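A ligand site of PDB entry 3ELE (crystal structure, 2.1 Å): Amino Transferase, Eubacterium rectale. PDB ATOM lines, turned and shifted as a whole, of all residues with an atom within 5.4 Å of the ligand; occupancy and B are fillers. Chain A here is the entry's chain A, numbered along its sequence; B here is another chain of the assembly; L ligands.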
ATOM      1  N   GLY A 107      17.608 -14.367 -17.359  1.00  0.00           N
ATOM      2  CA  GLY A 107      17.141 -13.147 -16.707  1.00  0.00           C
ATOM      3  C   GLY A 107      15.643 -12.943 -16.803  1.00  0.00           C
ATOM      4  O   GLY A 107      14.929 -13.677 -17.504  1.00  0.00           O
ATOM      5  N   ALA A 108      15.179 -11.931 -16.064  1.00  0.00           N
ATOM      6  CA  ALA A 108      13.786 -11.550 -15.980  1.00  0.00           C
ATOM      7  C   ALA A 108      13.196 -11.098 -17.311  1.00  0.00           C
ATOM      8  O   ALA A 108      12.037 -11.357 -17.548  1.00  0.00           O
ATOM      9  CB  ALA A 108      13.573 -10.475 -14.918  1.00  0.00           C
ATOM     10  N   ALA A 109      13.961 -10.411 -18.157  1.00  0.00           N
ATOM     11  CA  ALA A 109      13.478  -9.999 -19.500  1.00  0.00           C
ATOM     12  C   ALA A 109      13.129 -11.223 -20.345  1.00  0.00           C
ATOM     13  O   ALA A 109      12.190 -11.179 -21.119  1.00  0.00           O
ATOM     14  CB  ALA A 109      14.494  -9.152 -20.232  1.00  0.00           C
ATOM     15  N   ALA A 110      13.917 -12.292 -20.202  1.00  0.00           N
ATOM     16  CA  ALA A 110      13.654 -13.549 -20.900  1.00  0.00           C
ATOM     17  C   ALA A 110      12.403 -14.238 -20.295  1.00  0.00           C
ATOM     18  O   ALA A 110      11.583 -14.740 -21.027  1.00  0.00           O
ATOM     19  CB  ALA A 110      14.863 -14.458 -20.846  1.00  0.00           C
ATOM     20  N   LEU A 112       9.799 -12.816 -18.686  1.00  0.00           N
ATOM     21  CA  LEU A 112       8.609 -12.032 -19.115  1.00  0.00           C
ATOM     22  C   LEU A 112       8.259 -12.297 -20.566  1.00  0.00           C
ATOM     23  O   LEU A 112       7.096 -12.583 -20.886  1.00  0.00           O
ATOM     24  CB  LEU A 112       8.833 -10.539 -18.876  1.00  0.00           C
ATOM     25  CG  LEU A 112       8.930 -10.129 -17.390  1.00  0.00           C
ATOM     26  CD1 LEU A 112       9.506  -8.735 -17.244  1.00  0.00           C
ATOM     27  CD2 LEU A 112       7.575 -10.250 -16.699  1.00  0.00           C
ATOM     28  N   PHE A 134       7.200  -0.329 -15.145  1.00  0.00           N
ATOM     29  CA  PHE A 134       8.417  -0.529 -15.929  1.00  0.00           C
ATOM     30  C   PHE A 134       8.049  -0.453 -17.433  1.00  0.00           C
ATOM     31  O   PHE A 134       7.416  -1.384 -17.954  1.00  0.00           O
ATOM     32  CB  PHE A 134       8.991  -1.901 -15.558  1.00  0.00           C
ATOM     33  CG  PHE A 134      10.307  -2.254 -16.189  1.00  0.00           C
ATOM     34  CD1 PHE A 134      11.391  -1.379 -16.139  1.00  0.00           C
ATOM     35  CD2 PHE A 134      10.506  -3.530 -16.735  1.00  0.00           C
ATOM     36  CE1 PHE A 134      12.628  -1.742 -16.697  1.00  0.00           C
ATOM     37  CE2 PHE A 134      11.733  -3.906 -17.286  1.00  0.00           C
ATOM     38  CZ  PHE A 134      12.787  -2.998 -17.274  1.00  0.00           C
ATOM     39  N   TYR A 137       7.782  -3.326 -20.305  1.00  0.00           N
ATOM     40  CA  TYR A 137       6.639  -4.261 -20.442  1.00  0.00           C
ATOM     41  C   TYR A 137       5.929  -4.087 -21.768  1.00  0.00           C
ATOM     42  O   TYR A 137       5.528  -5.079 -22.362  1.00  0.00           O
ATOM     43  CB  TYR A 137       5.588  -4.106 -19.324  1.00  0.00           C
ATOM     44  CG  TYR A 137       6.050  -4.415 -17.906  1.00  0.00           C
ATOM     45  CD1 TYR A 137       7.021  -5.397 -17.644  1.00  0.00           C
ATOM     46  CD2 TYR A 137       5.426  -3.809 -16.818  1.00  0.00           C
ATOM     47  CE1 TYR A 137       7.403  -5.689 -16.340  1.00  0.00           C
ATOM     48  CE2 TYR A 137       5.780  -4.097 -15.532  1.00  0.00           C
ATOM     49  CZ  TYR A 137       6.784  -5.023 -15.283  1.00  0.00           C
ATOM     50  OH  TYR A 137       7.114  -5.286 -14.003  1.00  0.00           O
ATOM     51  N   ASN A 179       4.426  -6.114 -10.122  1.00  0.00           N
ATOM     52  CA  ASN A 179       5.847  -5.961  -9.826  1.00  0.00           C
ATOM     53  C   ASN A 179       5.903  -5.421  -8.415  1.00  0.00           C
ATOM     54  O   ASN A 179       5.675  -4.236  -8.206  1.00  0.00           O
ATOM     55  CB  ASN A 179       6.401  -5.025 -10.886  1.00  0.00           C
ATOM     56  CG  ASN A 179       7.834  -4.599 -10.664  1.00  0.00           C
ATOM     57  OD1 ASN A 179       8.127  -3.433 -10.908  1.00  0.00           O
ATOM     58  ND2 ASN A 179       8.725  -5.505 -10.239  1.00  0.00           N
ATOM     59  N   ASN A 183       9.288  -1.248  -9.320  1.00  0.00           N
ATOM     60  CA  ASN A 183      10.054  -0.260 -10.099  1.00  0.00           C
ATOM     61  C   ASN A 183       8.913   0.415 -10.916  1.00  0.00           C
ATOM     62  O   ASN A 183       8.296  -0.259 -11.758  1.00  0.00           O
ATOM     63  CB  ASN A 183      11.071  -0.919 -11.030  1.00  0.00           C
ATOM     64  CG  ASN A 183      11.760   0.073 -11.964  1.00  0.00           C
ATOM     65  OD1 ASN A 183      11.746   1.285 -11.710  1.00  0.00           O
ATOM     66  ND2 ASN A 183      12.377  -0.440 -13.023  1.00  0.00           N
ATOM     67  N   ASP A 217       6.331 -10.213 -11.618  1.00  0.00           N
ATOM     68  CA  ASP A 217       7.690  -9.769 -11.942  1.00  0.00           C
ATOM     69  C   ASP A 217       8.389  -9.495 -10.627  1.00  0.00           C
ATOM     70  O   ASP A 217       8.281  -8.385 -10.086  1.00  0.00           O
ATOM     71  CB  ASP A 217       7.621  -8.506 -12.831  1.00  0.00           C
ATOM     72  CG  ASP A 217       8.943  -8.096 -13.391  1.00  0.00           C
ATOM     73  OD1 ASP A 217       9.881  -8.910 -13.390  1.00  0.00           O
ATOM     74  OD2 ASP A 217       9.013  -6.962 -13.890  1.00  0.00           O
ATOM     75  N   PRO A 219      11.931  -9.548  -9.420  1.00  0.00           N
ATOM     76  CA  PRO A 219      13.386  -9.475  -9.185  1.00  0.00           C
ATOM     77  C   PRO A 219      13.820  -8.696  -7.928  1.00  0.00           C
ATOM     78  O   PRO A 219      14.942  -8.928  -7.454  1.00  0.00           O
ATOM     79  CB  PRO A 219      13.935  -8.832 -10.469  1.00  0.00           C
ATOM     80  CG  PRO A 219      12.817  -7.966 -10.964  1.00  0.00           C
ATOM     81  CD  PRO A 219      11.544  -8.748 -10.600  1.00  0.00           C
ATOM     82  N   TYR A 220      12.958  -7.808  -7.384  1.00  0.00           N
ATOM     83  CA  TYR A 220      13.241  -7.040  -6.145  1.00  0.00           C
ATOM     84  C   TYR A 220      12.721  -7.719  -4.863  1.00  0.00           C
ATOM     85  O   TYR A 220      12.796  -7.107  -3.789  1.00  0.00           O
ATOM     86  CB  TYR A 220      12.631  -5.614  -6.216  1.00  0.00           C
ATOM     87  CG  TYR A 220      13.136  -4.839  -7.401  1.00  0.00           C
ATOM     88  CD1 TYR A 220      14.394  -4.289  -7.381  1.00  0.00           C
ATOM     89  CD2 TYR A 220      12.368  -4.697  -8.555  1.00  0.00           C
ATOM     90  CE1 TYR A 220      14.889  -3.591  -8.463  1.00  0.00           C
ATOM     91  CE2 TYR A 220      12.869  -3.989  -9.667  1.00  0.00           C
ATOM     92  CZ  TYR A 220      14.149  -3.452  -9.600  1.00  0.00           C
ATOM     93  OH  TYR A 220      14.726  -2.755 -10.630  1.00  0.00           O
ATOM     94  N   SER A 245      14.736 -13.297 -11.265  1.00  0.00           N
ATOM     95  CA  SER A 245      16.117 -13.316 -11.689  1.00  0.00           C
ATOM     96  C   SER A 245      17.012 -12.970 -10.500  1.00  0.00           C
ATOM     97  O   SER A 245      16.541 -12.413  -9.516  1.00  0.00           O
ATOM     98  CB  SER A 245      16.381 -12.374 -12.857  1.00  0.00           C
ATOM     99  OG  SER A 245      16.497 -11.023 -12.447  1.00  0.00           O
ATOM    100  N   SER A 247      19.497 -10.842 -10.725  1.00  0.00           N
ATOM    101  CA  SER A 247      20.094  -9.563 -11.098  1.00  0.00           C
ATOM    102  C   SER A 247      20.242  -8.610  -9.898  1.00  0.00           C
ATOM    103  O   SER A 247      21.257  -7.928  -9.789  1.00  0.00           O
ATOM    104  CB  SER A 247      19.309  -8.890 -12.226  1.00  0.00           C
ATOM    105  OG  SER A 247      19.257  -9.739 -13.392  1.00  0.00           O
ATOM    106  N   LYS A 248      19.258  -8.601  -8.998  1.00  0.00           N
ATOM    107  CA  LYS A 248      19.276  -7.716  -7.810  1.00  0.00           C
ATOM    108  C   LYS A 248      19.687  -8.412  -6.522  1.00  0.00           C
ATOM    109  O   LYS A 248      20.451  -7.844  -5.711  1.00  0.00           O
ATOM    110  CB  LYS A 248      17.918  -7.045  -7.619  1.00  0.00           C
ATOM    111  CG  LYS A 248      17.658  -5.896  -8.566  1.00  0.00           C
ATOM    112  CD  LYS A 248      17.173  -6.324  -9.926  1.00  0.00           C
ATOM    113  CE  LYS A 248      17.302  -5.216 -10.956  1.00  0.00           C
ATOM    114  NZ  LYS A 248      16.850  -5.686 -12.286  1.00  0.00           N
ATOM    115  N   PRO A 253      23.334  -8.700 -12.726  1.00  0.00           N
ATOM    116  CA  PRO A 253      22.468  -8.330 -13.859  1.00  0.00           C
ATOM    117  C   PRO A 253      23.007  -8.668 -15.252  1.00  0.00           C
ATOM    118  O   PRO A 253      22.228  -8.979 -16.143  1.00  0.00           O
ATOM    119  CB  PRO A 253      22.286  -6.822 -13.696  1.00  0.00           C
ATOM    120  CG  PRO A 253      23.416  -6.370 -12.974  1.00  0.00           C
ATOM    121  CD  PRO A 253      23.782  -7.477 -12.021  1.00  0.00           C
ATOM    122  N   ARG A 256      22.745 -12.884 -16.599  1.00  0.00           N
ATOM    123  CA  ARG A 256      21.532 -13.400 -17.269  1.00  0.00           C
ATOM    124  C   ARG A 256      21.103 -14.767 -16.737  1.00  0.00           C
ATOM    125  O   ARG A 256      21.282 -15.789 -17.385  1.00  0.00           O
ATOM    126  CB  ARG A 256      21.736 -13.427 -18.818  1.00  0.00           C
ATOM    127  CG  ARG A 256      22.444 -12.215 -19.440  1.00  0.00           C
ATOM    128  CD  ARG A 256      21.902 -10.898 -18.944  1.00  0.00           C
ATOM    129  NE  ARG A 256      20.487 -10.723 -19.255  1.00  0.00           N
ATOM    130  CZ  ARG A 256      19.546 -10.173 -18.488  1.00  0.00           C
ATOM    131  NH1 ARG A 256      19.776  -9.794 -17.246  1.00  0.00           N
ATOM    132  NH2 ARG A 256      18.318 -10.075 -18.966  1.00  0.00           N
ATOM    133  N   TYR A 335      14.242   2.596  -5.715  1.00  0.00           N
ATOM    134  CA  TYR A 335      13.744   3.778  -6.383  1.00  0.00           C
ATOM    135  C   TYR A 335      12.833   4.562  -5.437  1.00  0.00           C
ATOM    136  O   TYR A 335      11.971   3.955  -4.773  1.00  0.00           O
ATOM    137  CB  TYR A 335      12.948   3.359  -7.608  1.00  0.00           C
ATOM    138  CG  TYR A 335      13.672   2.398  -8.497  1.00  0.00           C
ATOM    139  CD1 TYR A 335      14.709   2.824  -9.319  1.00  0.00           C
ATOM    140  CD2 TYR A 335      13.347   1.035  -8.495  1.00  0.00           C
ATOM    141  CE1 TYR A 335      15.404   1.924 -10.144  1.00  0.00           C
ATOM    142  CE2 TYR A 335      14.014   0.141  -9.297  1.00  0.00           C
ATOM    143  CZ  TYR A 335      15.047   0.586 -10.121  1.00  0.00           C
ATOM    144  OH  TYR A 335      15.713  -0.298 -10.933  1.00  0.00           O
ATOM    145  N   TYR B  72      25.420  -5.128 -15.987  1.00  0.00           N
ATOM    146  CA  TYR B  72      24.932  -5.037 -17.367  1.00  0.00           C
ATOM    147  C   TYR B  72      26.019  -4.390 -18.242  1.00  0.00           C
ATOM    148  O   TYR B  72      26.709  -3.484 -17.799  1.00  0.00           O
ATOM    149  CB  TYR B  72      23.701  -4.127 -17.499  1.00  0.00           C
ATOM    150  CG  TYR B  72      22.407  -4.589 -16.879  1.00  0.00           C
ATOM    151  CD1 TYR B  72      21.705  -5.696 -17.394  1.00  0.00           C
ATOM    152  CD2 TYR B  72      21.821  -3.875 -15.825  1.00  0.00           C
ATOM    153  CE1 TYR B  72      20.466  -6.109 -16.822  1.00  0.00           C
ATOM    154  CE2 TYR B  72      20.608  -4.272 -15.246  1.00  0.00           C
ATOM    155  CZ  TYR B  72      19.937  -5.383 -15.753  1.00  0.00           C
ATOM    156  OH  TYR B  72      18.774  -5.748 -15.151  1.00  0.00           O
ATOM    157  N   VAL B 286      19.116  -8.637 -23.322  1.00  0.00           N
ATOM    158  CA  VAL B 286      19.550  -7.409 -22.651  1.00  0.00           C
ATOM    159  C   VAL B 286      21.058  -7.227 -22.922  1.00  0.00           C
ATOM    160  O   VAL B 286      21.491  -6.165 -23.293  1.00  0.00           O
ATOM    161  CB  VAL B 286      19.260  -7.473 -21.144  1.00  0.00           C
ATOM    162  CG1 VAL B 286      19.895  -6.291 -20.390  1.00  0.00           C
ATOM    163  CG2 VAL B 286      17.752  -7.504 -20.918  1.00  0.00           C
HETATM  164  N1  LIG L   1      11.547  -6.075 -14.028  1.00  0.00           N
HETATM  165  C1  LIG L   1      11.756  -4.843 -13.386  1.00  0.00           C
HETATM  166  C2  LIG L   1      10.620  -4.184 -12.692  1.00  0.00           C
HETATM  167  C3  LIG L   1      13.041  -4.258 -13.381  1.00  0.00           C
HETATM  168  O1  LIG L   1      13.260  -3.065 -12.745  1.00  0.00           O
HETATM  169  C4  LIG L   1      14.114  -4.888 -14.060  1.00  0.00           C
HETATM  170  C5  LIG L   1      15.299  -3.998 -14.376  1.00  0.00           C
HETATM  171  O2  LIG L   1      15.302  -3.324 -15.411  1.00  0.00           O
HETATM  172  C6  LIG L   1      13.876  -6.136 -14.700  1.00  0.00           C
HETATM  173  C7  LIG L   1      12.583  -6.721 -14.676  1.00  0.00           C
HETATM  174  C8  LIG L   1      14.937  -6.888 -15.473  1.00  0.00           C
HETATM  175  O3  LIG L   1      15.658  -7.803 -14.710  1.00  0.00           O
HETATM  176  P1  LIG L   1      16.713  -8.739 -15.471  1.00  0.00           P
HETATM  177  O4  LIG L   1      16.756 -10.095 -14.815  1.00  0.00           O
HETATM  178  O5  LIG L   1      18.088  -8.147 -15.329  1.00  0.00           O
HETATM  179  O6  LIG L   1      16.382  -8.898 -16.920  1.00  0.00           O
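ND2 of Asn 183 is in hydrogen-bond range of O1 of the ligand (2.8 Å). The side-chain hydroxyl (OG) of Ser 247 lies within hydrogen-bond range of an oxygen (O5) of the ligand (2.8 Å). An oxygen (O6) of the ligand is in hydrogen-bond range of the backbone NH (N) of Ala 109 (3.1 Å). The backbone NH (N) of Ala 108 lies within hydrogen-bond range of an oxygen (O4) of the ligand (2.7 Å). The side-chain hydroxyl (OG) of Ser 245 is in hydrogen-bond range of an oxygen (O4) of the ligand (2.6 Å). O1 of the ligand is in hydrogen-bond range of OH of Tyr 220 (2.6 Å). NZ of Lys 248 sits close to O3 of the ligand (3.4 Å). An oxygen (O5) of the ligand lies within salt-bridge range of the guanidinium group (NH1) of Arg 256, 3.0 Å away. OD2 of Asp 217 lies within hydrogen-bond range of N1 of the ligand, at 2.7 Å. O5 of the ligand sits at hydrogen-bond distance from OH of Tyr 72 of chain B, at 2.5 Å.
CA of Gly 107 touches O4 of the ligand (3.6 Å). Phe 134 touches the ligand (CZ to O2, 3.1 Å). Tyr 137 touches the ligand (OH to C2, 3.9 Å). Asn 179 touches the ligand. CG of Pro 219 touches N1 of the ligand, 3.8 Å away. Hydrophobic or aromatic side chains that line the ligand: Ala 108, Ala 109, Phe 134, Pro 219, Tyr 220 and Tyr 72 of chain B. 15 residues have an atom within 4 Å of the ligand: Gly 107, Ala 108, Ala 109, Phe 134, Tyr 137, Asn 179, Asn 183, Asp 217, Pro 219, Tyr 220, Ser 245, Ser 247, Lys 248, Arg 256 and Tyr 72 of chain B. The nearest printed residue that does not touch the ligand is Tyr 335 (4.1 Å).
OD1 of Asn 179 sits at hydrogen-bond distance from N of Asn 183. The side-chain hydroxyl (OH) of Tyr 72 of chain B is in hydrogen-bond range of the side-chain amino group (NZ) of Lys 248. The side-chain carboxylate (OD2) of Asp 217 sits at hydrogen-bond distance from the side-chain hydroxyl (OH) of Tyr 137, 2.5 Å away. ND2 of Asn 179 is in hydrogen-bond range of O of Asp 217 (2.9 Å). The guanidinium group (NH1) of Arg 256 lies within hydrogen-bond range of the backbone carbonyl oxygen (O) of Pro 253, at 2.8 Å. The side-chain hydroxyl (OH) of Tyr 220 is in hydrogen-bond range of the side-chain hydroxyl (OH) of Tyr 335, 2.7 Å away. The side-chain hydroxyl (OG) of Ser 245 is in hydrogen-bond range of the side-chain hydroxyl (OG) of Ser 247 (3.2 Å).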
